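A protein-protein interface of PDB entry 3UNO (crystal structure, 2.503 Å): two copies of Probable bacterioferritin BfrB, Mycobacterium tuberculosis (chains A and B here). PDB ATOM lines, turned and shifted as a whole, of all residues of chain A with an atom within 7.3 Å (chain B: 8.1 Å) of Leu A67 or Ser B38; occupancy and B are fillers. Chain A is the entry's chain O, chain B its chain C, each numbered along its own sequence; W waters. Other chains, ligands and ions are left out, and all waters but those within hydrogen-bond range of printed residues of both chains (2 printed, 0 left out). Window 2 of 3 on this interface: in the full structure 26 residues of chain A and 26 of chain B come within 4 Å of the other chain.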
ATOM      1  N   MET A  60     -11.630  -8.552  -8.009  1.00  0.00           N
ATOM      2  CA  MET A  60     -11.166  -9.706  -8.763  1.00  0.00           C
ATOM      3  C   MET A  60     -11.168  -9.419 -10.252  1.00  0.00           C
ATOM      4  O   MET A  60     -10.428 -10.067 -11.006  1.00  0.00           O
ATOM      5  CB  MET A  60     -11.971 -10.944  -8.407  1.00  0.00           C
ATOM      6  CG  MET A  60     -11.812 -11.439  -6.931  1.00  0.00           C
ATOM      7  SD  MET A  60     -10.073 -11.664  -6.466  1.00  0.00           S
ATOM      8  CE  MET A  60      -9.705 -13.299  -7.227  1.00  0.00           C
ATOM      9  N   MET A  61     -11.976  -8.447 -10.690  1.00  0.00           N
ATOM     10  CA  MET A  61     -11.912  -8.027 -12.113  1.00  0.00           C
ATOM     11  C   MET A  61     -10.616  -7.271 -12.418  1.00  0.00           C
ATOM     12  O   MET A  61     -10.048  -7.367 -13.525  1.00  0.00           O
ATOM     13  CB  MET A  61     -13.111  -7.194 -12.550  1.00  0.00           C
ATOM     14  CG  MET A  61     -14.406  -7.928 -12.390  1.00  0.00           C
ATOM     15  SD  MET A  61     -15.776  -6.766 -12.561  1.00  0.00           S
ATOM     16  CE  MET A  61     -17.223  -7.799 -12.145  1.00  0.00           C
ATOM     17  N   LEU A  62     -10.154  -6.524 -11.419  1.00  0.00           N
ATOM     18  CA  LEU A  62      -8.890  -5.807 -11.514  1.00  0.00           C
ATOM     19  C   LEU A  62      -7.732  -6.816 -11.543  1.00  0.00           C
ATOM     20  O   LEU A  62      -6.817  -6.716 -12.386  1.00  0.00           O
ATOM     21  CB  LEU A  62      -8.739  -4.814 -10.359  1.00  0.00           C
ATOM     22  CG  LEU A  62      -9.808  -3.730 -10.317  1.00  0.00           C
ATOM     23  CD1 LEU A  62      -9.700  -2.894  -9.008  1.00  0.00           C
ATOM     24  CD2 LEU A  62      -9.681  -2.781 -11.526  1.00  0.00           C
ATOM     25  N   VAL A  63      -7.778  -7.804 -10.651  1.00  0.00           N
ATOM     26  CA  VAL A  63      -6.759  -8.846 -10.640  1.00  0.00           C
ATOM     27  C   VAL A  63      -6.702  -9.477 -12.023  1.00  0.00           C
ATOM     28  O   VAL A  63      -5.628  -9.604 -12.624  1.00  0.00           O
ATOM     29  CB  VAL A  63      -7.074  -9.922  -9.553  1.00  0.00           C
ATOM     30  CG1 VAL A  63      -6.119 -11.111  -9.675  1.00  0.00           C
ATOM     31  CG2 VAL A  63      -6.991  -9.295  -8.128  1.00  0.00           C
ATOM     32  N   GLN A  64      -7.868  -9.892 -12.517  1.00  0.00           N
ATOM     33  CA  GLN A  64      -7.968 -10.530 -13.826  1.00  0.00           C
ATOM     34  C   GLN A  64      -7.312  -9.673 -14.925  1.00  0.00           C
ATOM     35  O   GLN A  64      -6.637 -10.184 -15.834  1.00  0.00           O
ATOM     36  CB  GLN A  64      -9.447 -10.803 -14.180  1.00  0.00           C
ATOM     37  CG  GLN A  64      -9.668 -11.605 -15.447  1.00  0.00           C
ATOM     38  CD  GLN A  64      -9.078 -13.005 -15.361  1.00  0.00           C
ATOM     39  OE1 GLN A  64      -9.426 -13.797 -14.475  1.00  0.00           O
ATOM     40  NE2 GLN A  64      -8.188 -13.324 -16.303  1.00  0.00           N
ATOM     41  N   HIS A  65      -7.500  -8.363 -14.843  1.00  0.00           N
ATOM     42  CA  HIS A  65      -6.981  -7.492 -15.896  1.00  0.00           C
ATOM     43  C   HIS A  65      -5.448  -7.550 -15.921  1.00  0.00           C
ATOM     44  O   HIS A  65      -4.826  -7.684 -16.980  1.00  0.00           O
ATOM     45  CB  HIS A  65      -7.476  -6.059 -15.719  1.00  0.00           C
ATOM     46  CG  HIS A  65      -6.942  -5.099 -16.739  1.00  0.00           C
ATOM     47  ND1 HIS A  65      -7.476  -4.989 -18.014  1.00  0.00           N
ATOM     48  CD2 HIS A  65      -5.946  -4.189 -16.662  1.00  0.00           C
ATOM     49  CE1 HIS A  65      -6.810  -4.056 -18.675  1.00  0.00           C
ATOM     50  NE2 HIS A  65      -5.874  -3.555 -17.885  1.00  0.00           N
ATOM     51  N   LEU A  66      -4.837  -7.481 -14.748  1.00  0.00           N
ATOM     52  CA  LEU A  66      -3.383  -7.613 -14.681  1.00  0.00           C
ATOM     53  C   LEU A  66      -2.912  -8.999 -15.147  1.00  0.00           C
ATOM     54  O   LEU A  66      -1.906  -9.109 -15.887  1.00  0.00           O
ATOM     55  CB  LEU A  66      -2.870  -7.284 -13.275  1.00  0.00           C
ATOM     56  CG  LEU A  66      -3.135  -5.824 -12.826  1.00  0.00           C
ATOM     57  CD1 LEU A  66      -2.541  -5.602 -11.411  1.00  0.00           C
ATOM     58  CD2 LEU A  66      -2.541  -4.847 -13.817  1.00  0.00           C
ATOM     59  N   LEU A  67      -3.633 -10.046 -14.721  1.00  0.00           N
ATOM     60  CA  LEU A  67      -3.383 -11.408 -15.202  1.00  0.00           C
ATOM     61  C   LEU A  67      -3.429 -11.451 -16.732  1.00  0.00           C
ATOM     62  O   LEU A  67      -2.513 -11.977 -17.369  1.00  0.00           O
ATOM     63  CB  LEU A  67      -4.421 -12.388 -14.642  1.00  0.00           C
ATOM     64  CG  LEU A  67      -4.218 -12.863 -13.191  1.00  0.00           C
ATOM     65  CD1 LEU A  67      -5.387 -13.802 -12.744  1.00  0.00           C
ATOM     66  CD2 LEU A  67      -2.848 -13.602 -13.028  1.00  0.00           C
ATOM     67  N   ASP A  68      -4.494 -10.898 -17.319  1.00  0.00           N
ATOM     68  CA  ASP A  68      -4.641 -10.901 -18.774  1.00  0.00           C
ATOM     69  C   ASP A  68      -3.472 -10.204 -19.484  1.00  0.00           C
ATOM     70  O   ASP A  68      -3.112 -10.560 -20.601  1.00  0.00           O
ATOM     71  CB  ASP A  68      -5.957 -10.222 -19.210  1.00  0.00           C
ATOM     72  CG  ASP A  68      -7.188 -11.043 -18.903  1.00  0.00           C
ATOM     73  OD1 ASP A  68      -7.087 -12.277 -18.698  1.00  0.00           O
ATOM     74  OD2 ASP A  68      -8.275 -10.435 -18.869  1.00  0.00           O
ATOM     75  N   ARG A  69      -2.869  -9.224 -18.815  1.00  0.00           N
ATOM     76  CA  ARG A  69      -1.791  -8.434 -19.411  1.00  0.00           C
ATOM     77  C   ARG A  69      -0.413  -8.878 -18.985  1.00  0.00           C
ATOM     78  O   ARG A  69       0.575  -8.224 -19.318  1.00  0.00           O
ATOM     79  CB  ARG A  69      -2.012  -6.955 -19.119  1.00  0.00           C
ATOM     80  CG  ARG A  69      -3.266  -6.478 -19.857  1.00  0.00           C
ATOM     81  CD  ARG A  69      -3.553  -5.019 -19.620  1.00  0.00           C
ATOM     82  NE  ARG A  69      -2.479  -4.181 -20.125  1.00  0.00           N
ATOM     83  CZ  ARG A  69      -2.374  -2.876 -19.895  1.00  0.00           C
ATOM     84  NH1 ARG A  69      -3.317  -2.258 -19.173  1.00  0.00           N
ATOM     85  NH2 ARG A  69      -1.328  -2.208 -20.398  1.00  0.00           N
ATOM     86  N   ASP A  70      -0.351  -9.985 -18.240  1.00  0.00           N
ATOM     87  CA  ASP A  70       0.932 -10.509 -17.736  1.00  0.00           C
ATOM     88  C   ASP A  70       1.692  -9.471 -16.893  1.00  0.00           C
ATOM     89  O   ASP A  70       2.924  -9.397 -16.934  1.00  0.00           O
ATOM     90  CB  ASP A  70       1.835 -11.034 -18.865  1.00  0.00           C
ATOM     91  CG  ASP A  70       2.897 -12.070 -18.362  1.00  0.00           C
ATOM     92  OD1 ASP A  70       2.758 -12.619 -17.227  1.00  0.00           O
ATOM     93  OD2 ASP A  70       3.870 -12.345 -19.116  1.00  0.00           O
ATOM     94  N   LEU A  71       0.944  -8.665 -16.140  1.00  0.00           N
ATOM     95  CA  LEU A  71       1.512  -7.673 -15.238  1.00  0.00           C
ATOM     96  C   LEU A  71       1.441  -8.251 -13.825  1.00  0.00           C
ATOM     97  O   LEU A  71       0.445  -8.913 -13.471  1.00  0.00           O
ATOM     98  CB  LEU A  71       0.705  -6.386 -15.332  1.00  0.00           C
ATOM     99  CG  LEU A  71       0.866  -5.657 -16.666  1.00  0.00           C
ATOM    100  CD1 LEU A  71      -0.094  -4.419 -16.767  1.00  0.00           C
ATOM    101  CD2 LEU A  71       2.336  -5.248 -16.843  1.00  0.00           C
ATOM    102  N   ARG A  72       2.482  -8.026 -13.020  1.00  0.00           N
ATOM    103  CA  ARG A  72       2.555  -8.645 -11.688  1.00  0.00           C
ATOM    104  C   ARG A  72       1.383  -8.164 -10.823  1.00  0.00           C
ATOM    105  O   ARG A  72       1.000  -6.983 -10.846  1.00  0.00           O
ATOM    106  CB  ARG A  72       3.872  -8.290 -10.996  1.00  0.00           C
ATOM    107  CG  ARG A  72       3.974  -8.765  -9.557  1.00  0.00           C
ATOM    108  CD  ARG A  72       5.434  -9.108  -9.179  1.00  0.00           C
ATOM    109  NE  ARG A  72       5.798 -10.471  -9.576  1.00  0.00           N
ATOM    110  CZ  ARG A  72       6.848 -10.780 -10.336  1.00  0.00           C
ATOM    111  NH1 ARG A  72       7.657  -9.824 -10.793  1.00  0.00           N
ATOM    112  NH2 ARG A  72       7.093 -12.048 -10.642  1.00  0.00           N
ATOM    113  N   VAL A  73       0.804  -9.077 -10.061  1.00  0.00           N
ATOM    114  CA  VAL A  73      -0.299  -8.692  -9.203  1.00  0.00           C
ATOM    115  C   VAL A  73      -0.124  -9.378  -7.851  1.00  0.00           C
ATOM    116  O   VAL A  73       0.237 -10.552  -7.787  1.00  0.00           O
ATOM    117  CB  VAL A  73      -1.682  -9.019  -9.842  1.00  0.00           C
ATOM    118  CG1 VAL A  73      -1.688 -10.452 -10.468  1.00  0.00           C
ATOM    119  CG2 VAL A  73      -2.821  -8.831  -8.820  1.00  0.00           C
ATOM    120  N   ALA A 177     -11.510 -12.761 -11.829  1.00  0.00           N
ATOM    121  CA  ALA A 177     -10.662 -13.943 -11.570  1.00  0.00           C
ATOM    122  C   ALA A 177     -11.416 -14.803 -10.590  1.00  0.00           C
ATOM    123  O   ALA A 177     -11.890 -14.299  -9.550  1.00  0.00           O
ATOM    124  CB  ALA A 177      -9.348 -13.529 -10.947  1.00  0.00           C
ATOM    125  N   GLY A 178     -11.533 -16.086 -10.896  1.00  0.00           N
ATOM    126  CA  GLY A 178     -12.277 -16.976 -10.030  1.00  0.00           C
ATOM    127  C   GLY A 178     -13.784 -16.991 -10.273  1.00  0.00           C
ATOM    128  O   GLY A 178     -14.533 -17.699  -9.572  1.00  0.00           O
ATOM    129  N   ALA B  31      -4.566 -15.601  -2.822  1.00  0.00           N
ATOM    130  CA  ALA B  31      -3.190 -15.396  -3.334  1.00  0.00           C
ATOM    131  C   ALA B  31      -2.683 -16.642  -4.055  1.00  0.00           C
ATOM    132  O   ALA B  31      -2.077 -16.544  -5.127  1.00  0.00           O
ATOM    133  CB  ALA B  31      -2.246 -15.036  -2.223  1.00  0.00           C
ATOM    134  N   ILE B  32      -2.966 -17.809  -3.479  1.00  0.00           N
ATOM    135  CA  ILE B  32      -2.533 -19.065  -4.062  1.00  0.00           C
ATOM    136  C   ILE B  32      -3.311 -19.356  -5.356  1.00  0.00           C
ATOM    137  O   ILE B  32      -2.732 -19.860  -6.306  1.00  0.00           O
ATOM    138  CB  ILE B  32      -2.674 -20.237  -3.038  1.00  0.00           C
ATOM    139  CG1 ILE B  32      -1.575 -20.095  -1.964  1.00  0.00           C
ATOM    140  CG2 ILE B  32      -2.601 -21.612  -3.767  1.00  0.00           C
ATOM    141  CD1 ILE B  32      -1.737 -21.062  -0.805  1.00  0.00           C
ATOM    142  N   ALA B  33      -4.607 -19.048  -5.379  1.00  0.00           N
ATOM    143  CA  ALA B  33      -5.453 -19.278  -6.548  1.00  0.00           C
ATOM    144  C   ALA B  33      -4.907 -18.449  -7.688  1.00  0.00           C
ATOM    145  O   ALA B  33      -4.775 -18.959  -8.799  1.00  0.00           O
ATOM    146  CB  ALA B  33      -6.962 -18.876  -6.247  1.00  0.00           C
ATOM    147  N   VAL B  34      -4.608 -17.170  -7.393  1.00  0.00           N
ATOM    148  CA  VAL B  34      -4.083 -16.217  -8.367  1.00  0.00           C
ATOM    149  C   VAL B  34      -2.712 -16.629  -8.897  1.00  0.00           C
ATOM    150  O   VAL B  34      -2.443 -16.527 -10.117  1.00  0.00           O
ATOM    151  CB  VAL B  34      -4.086 -14.771  -7.817  1.00  0.00           C
ATOM    152  CG1 VAL B  34      -3.314 -13.828  -8.774  1.00  0.00           C
ATOM    153  CG2 VAL B  34      -5.561 -14.270  -7.661  1.00  0.00           C
ATOM    154  N   TYR B  35      -1.844 -17.077  -7.993  1.00  0.00           N
ATOM    155  CA  TYR B  35      -0.550 -17.635  -8.395  1.00  0.00           C
ATOM    156  C   TYR B  35      -0.717 -18.742  -9.450  1.00  0.00           C
ATOM    157  O   TYR B  35      -0.132 -18.673 -10.543  1.00  0.00           O
ATOM    158  CB  TYR B  35       0.247 -18.139  -7.162  1.00  0.00           C
ATOM    159  CG  TYR B  35       1.396 -19.040  -7.557  1.00  0.00           C
ATOM    160  CD1 TYR B  35       2.487 -18.536  -8.285  1.00  0.00           C
ATOM    161  CD2 TYR B  35       1.383 -20.397  -7.240  1.00  0.00           C
ATOM    162  CE1 TYR B  35       3.557 -19.364  -8.657  1.00  0.00           C
ATOM    163  CE2 TYR B  35       2.418 -21.234  -7.650  1.00  0.00           C
ATOM    164  CZ  TYR B  35       3.526 -20.708  -8.328  1.00  0.00           C
ATOM    165  OH  TYR B  35       4.559 -21.561  -8.711  1.00  0.00           O
ATOM    166  N   PHE B  36      -1.524 -19.756  -9.129  1.00  0.00           N
ATOM    167  CA  PHE B  36      -1.873 -20.846 -10.087  1.00  0.00           C
ATOM    168  C   PHE B  36      -2.432 -20.335 -11.417  1.00  0.00           C
ATOM    169  O   PHE B  36      -1.982 -20.746 -12.472  1.00  0.00           O
ATOM    170  CB  PHE B  36      -2.866 -21.836  -9.439  1.00  0.00           C
ATOM    171  CG  PHE B  36      -2.244 -22.696  -8.343  1.00  0.00           C
ATOM    172  CD1 PHE B  36      -0.921 -23.087  -8.424  1.00  0.00           C
ATOM    173  CD2 PHE B  36      -2.981 -23.101  -7.236  1.00  0.00           C
ATOM    174  CE1 PHE B  36      -0.350 -23.881  -7.429  1.00  0.00           C
ATOM    175  CE2 PHE B  36      -2.419 -23.876  -6.229  1.00  0.00           C
ATOM    176  CZ  PHE B  36      -1.099 -24.276  -6.345  1.00  0.00           C
ATOM    177  N   ASP B  37      -3.432 -19.453 -11.343  1.00  0.00           N
ATOM    178  CA  ASP B  37      -4.025 -18.808 -12.519  1.00  0.00           C
ATOM    179  C   ASP B  37      -2.924 -18.221 -13.393  1.00  0.00           C
ATOM    180  O   ASP B  37      -2.917 -18.412 -14.611  1.00  0.00           O
ATOM    181  CB  ASP B  37      -4.961 -17.691 -12.049  1.00  0.00           C
ATOM    182  CG  ASP B  37      -5.999 -17.284 -13.097  1.00  0.00           C
ATOM    183  OD1 ASP B  37      -5.648 -17.138 -14.298  1.00  0.00           O
ATOM    184  OD2 ASP B  37      -7.191 -17.113 -12.700  1.00  0.00           O
ATOM    185  N   SER B  38      -1.970 -17.528 -12.777  1.00  0.00           N
ATOM    186  CA  SER B  38      -0.906 -16.870 -13.568  1.00  0.00           C
ATOM    187  C   SER B  38       0.075 -17.892 -14.142  1.00  0.00           C
ATOM    188  O   SER B  38       0.716 -17.650 -15.173  1.00  0.00           O
ATOM    189  CB  SER B  38      -0.123 -15.858 -12.758  1.00  0.00           C
ATOM    190  OG  SER B  38       0.652 -16.535 -11.799  1.00  0.00           O
ATOM    191  N   GLU B  39       0.199 -19.032 -13.472  1.00  0.00           N
ATOM    192  CA  GLU B  39       0.989 -20.129 -14.011  1.00  0.00           C
ATOM    193  C   GLU B  39       0.230 -20.953 -15.043  1.00  0.00           C
ATOM    194  O   GLU B  39       0.738 -21.974 -15.490  1.00  0.00           O
ATOM    195  CB  GLU B  39       1.430 -21.073 -12.874  1.00  0.00           C
ATOM    196  CG  GLU B  39       2.574 -20.533 -12.004  1.00  0.00           C
ATOM    197  CD  GLU B  39       3.823 -20.134 -12.822  1.00  0.00           C
ATOM    198  OE1 GLU B  39       4.249 -20.896 -13.713  1.00  0.00           O
ATOM    199  OE2 GLU B  39       4.397 -19.053 -12.564  1.00  0.00           O
ATOM    200  N   ASP B  40      -0.995 -20.548 -15.392  1.00  0.00           N
ATOM    201  CA  ASP B  40      -1.859 -21.365 -16.274  1.00  0.00           C
ATOM    202  C   ASP B  40      -2.081 -22.776 -15.777  1.00  0.00           C
ATOM    203  O   ASP B  40      -1.900 -23.712 -16.522  1.00  0.00           O
ATOM    204  CB  ASP B  40      -1.270 -21.437 -17.673  1.00  0.00           C
ATOM    205  CG  ASP B  40      -1.043 -20.048 -18.265  1.00  0.00           C
ATOM    206  OD1 ASP B  40      -2.049 -19.272 -18.363  1.00  0.00           O
ATOM    207  OD2 ASP B  40       0.150 -19.729 -18.539  1.00  0.00           O
ATOM    208  N   LEU B  41      -2.477 -22.911 -14.513  1.00  0.00           N
ATOM    209  CA  LEU B  41      -2.946 -24.158 -13.964  1.00  0.00           C
ATOM    210  C   LEU B  41      -4.378 -23.907 -13.474  1.00  0.00           C
ATOM    211  O   LEU B  41      -4.656 -23.757 -12.231  1.00  0.00           O
ATOM    212  CB  LEU B  41      -2.051 -24.604 -12.805  1.00  0.00           C
ATOM    213  CG  LEU B  41      -0.589 -24.792 -13.145  1.00  0.00           C
ATOM    214  CD1 LEU B  41       0.319 -24.871 -11.921  1.00  0.00           C
ATOM    215  CD2 LEU B  41      -0.449 -26.078 -13.984  1.00  0.00           C
ATOM    216  N   PRO B  42      -5.300 -23.835 -14.449  1.00  0.00           N
ATOM    217  CA  PRO B  42      -6.709 -23.447 -14.189  1.00  0.00           C
ATOM    218  C   PRO B  42      -7.487 -24.412 -13.265  1.00  0.00           C
ATOM    219  O   PRO B  42      -8.326 -23.959 -12.454  1.00  0.00           O
ATOM    220  CB  PRO B  42      -7.355 -23.348 -15.591  1.00  0.00           C
ATOM    221  CG  PRO B  42      -6.394 -24.211 -16.518  1.00  0.00           C
ATOM    222  CD  PRO B  42      -5.003 -24.092 -15.880  1.00  0.00           C
ATOM    223  N   ALA B  45      -6.233 -23.522  -9.907  1.00  0.00           N
ATOM    224  CA  ALA B  45      -6.697 -22.172  -9.601  1.00  0.00           C
ATOM    225  C   ALA B  45      -8.160 -22.205  -9.168  1.00  0.00           C
ATOM    226  O   ALA B  45      -8.522 -21.617  -8.138  1.00  0.00           O
ATOM    227  CB  ALA B  45      -6.501 -21.229 -10.826  1.00  0.00           C
ATOM    228  N   TYR B  49      -9.748 -20.865  -5.613  1.00  0.00           N
ATOM    229  CA  TYR B  49     -10.781 -19.812  -5.564  1.00  0.00           C
ATOM    230  C   TYR B  49     -11.958 -20.312  -4.719  1.00  0.00           C
ATOM    231  O   TYR B  49     -12.560 -19.581  -3.908  1.00  0.00           O
ATOM    232  CB  TYR B  49     -11.261 -19.435  -6.978  1.00  0.00           C
ATOM    233  CG  TYR B  49     -10.276 -18.624  -7.795  1.00  0.00           C
ATOM    234  CD1 TYR B  49      -9.784 -17.410  -7.330  1.00  0.00           C
ATOM    235  CD2 TYR B  49      -9.819 -19.082  -9.004  1.00  0.00           C
ATOM    236  CE1 TYR B  49      -8.886 -16.647  -8.086  1.00  0.00           C
ATOM    237  CE2 TYR B  49      -8.932 -18.324  -9.778  1.00  0.00           C
ATOM    238  CZ  TYR B  49      -8.474 -17.120  -9.317  1.00  0.00           C
ATOM    239  OH  TYR B  49      -7.584 -16.386 -10.087  1.00  0.00           O
ATOM    240  N   ASN B  83       2.569 -14.082  -1.733  1.00  0.00           N
ATOM    241  CA  ASN B  83       2.231 -14.113  -3.159  1.00  0.00           C
ATOM    242  C   ASN B  83       3.277 -14.830  -4.047  1.00  0.00           C
ATOM    243  O   ASN B  83       2.953 -15.264  -5.166  1.00  0.00           O
ATOM    244  CB  ASN B  83       1.923 -12.688  -3.685  1.00  0.00           C
ATOM    245  CG  ASN B  83       0.517 -12.169  -3.254  1.00  0.00           C
ATOM    246  OD1 ASN B  83      -0.496 -12.511  -3.882  1.00  0.00           O
ATOM    247  ND2 ASN B  83       0.462 -11.334  -2.208  1.00  0.00           N
HETATM  248  O   HOH W   1      -6.841 -15.942 -16.311  1.00  0.00           O
HETATM  249  O   HOH W   2      -9.198 -16.308 -13.821  1.00  0.00           O
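The side-chain carboxylate (OD2) of Asp B37 is in hydrogen-bond range of the side-chain hydroxyl (OH) of Tyr B49. The backbone carbonyl oxygen (O) of Met A60 lies within hydrogen-bond range of the backbone NH (N) of Ala A177, 3.0 Å away. The backbone carbonyl oxygen of Tyr B35 lies within hydrogen-bond range of the side-chain hydroxyl of Ser B38 (2.6 Å).
Of the 16 printed residues of chain A, 5 touch a printed residue of chain B. Hydrophobic or aromatic side chains of chain A that line the printed part of chain B: Met A60, Val A63, Leu A67 and Ala A177. Of the 15 printed residues of chain B, 4 touch a printed residue of chain A. Among the printed residues, 6 pairs touch across the chains. Among the printed residues, no Asp or Glu carboxylate lies within 4 Å of a Lys or Arg side-chain nitrogen of the other chain.
No position is printed for both chains.
Printed residues of chain B within 4 Å of Met A60: Tyr B49. Of the printed residues of chain B, Leu A67 touches Asp B37 and Ser B38. Printed residues of chain A within 4 Å of Val B34: Val A63. Ser B38 touches one residue of chain A.
Water W2 bridges the side-chain carboxylate (OD2) of Asp B37 (2.4 Å) and the side-chain amide oxygen (OE1) of Gln A64 (2.6 Å). Water W1 lies within hydrogen-bond range of OD1 of Asp B37 and NE2 of Gln A64.
Among the printed residues, merely in contact across the chains: Gly A178 with Tyr B49, Ala A177 with Tyr B49, Leu A67 with Ser B38, Met A60 with Tyr B49, Leu A67 with Asp B37 and Val A63 with Val B34.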
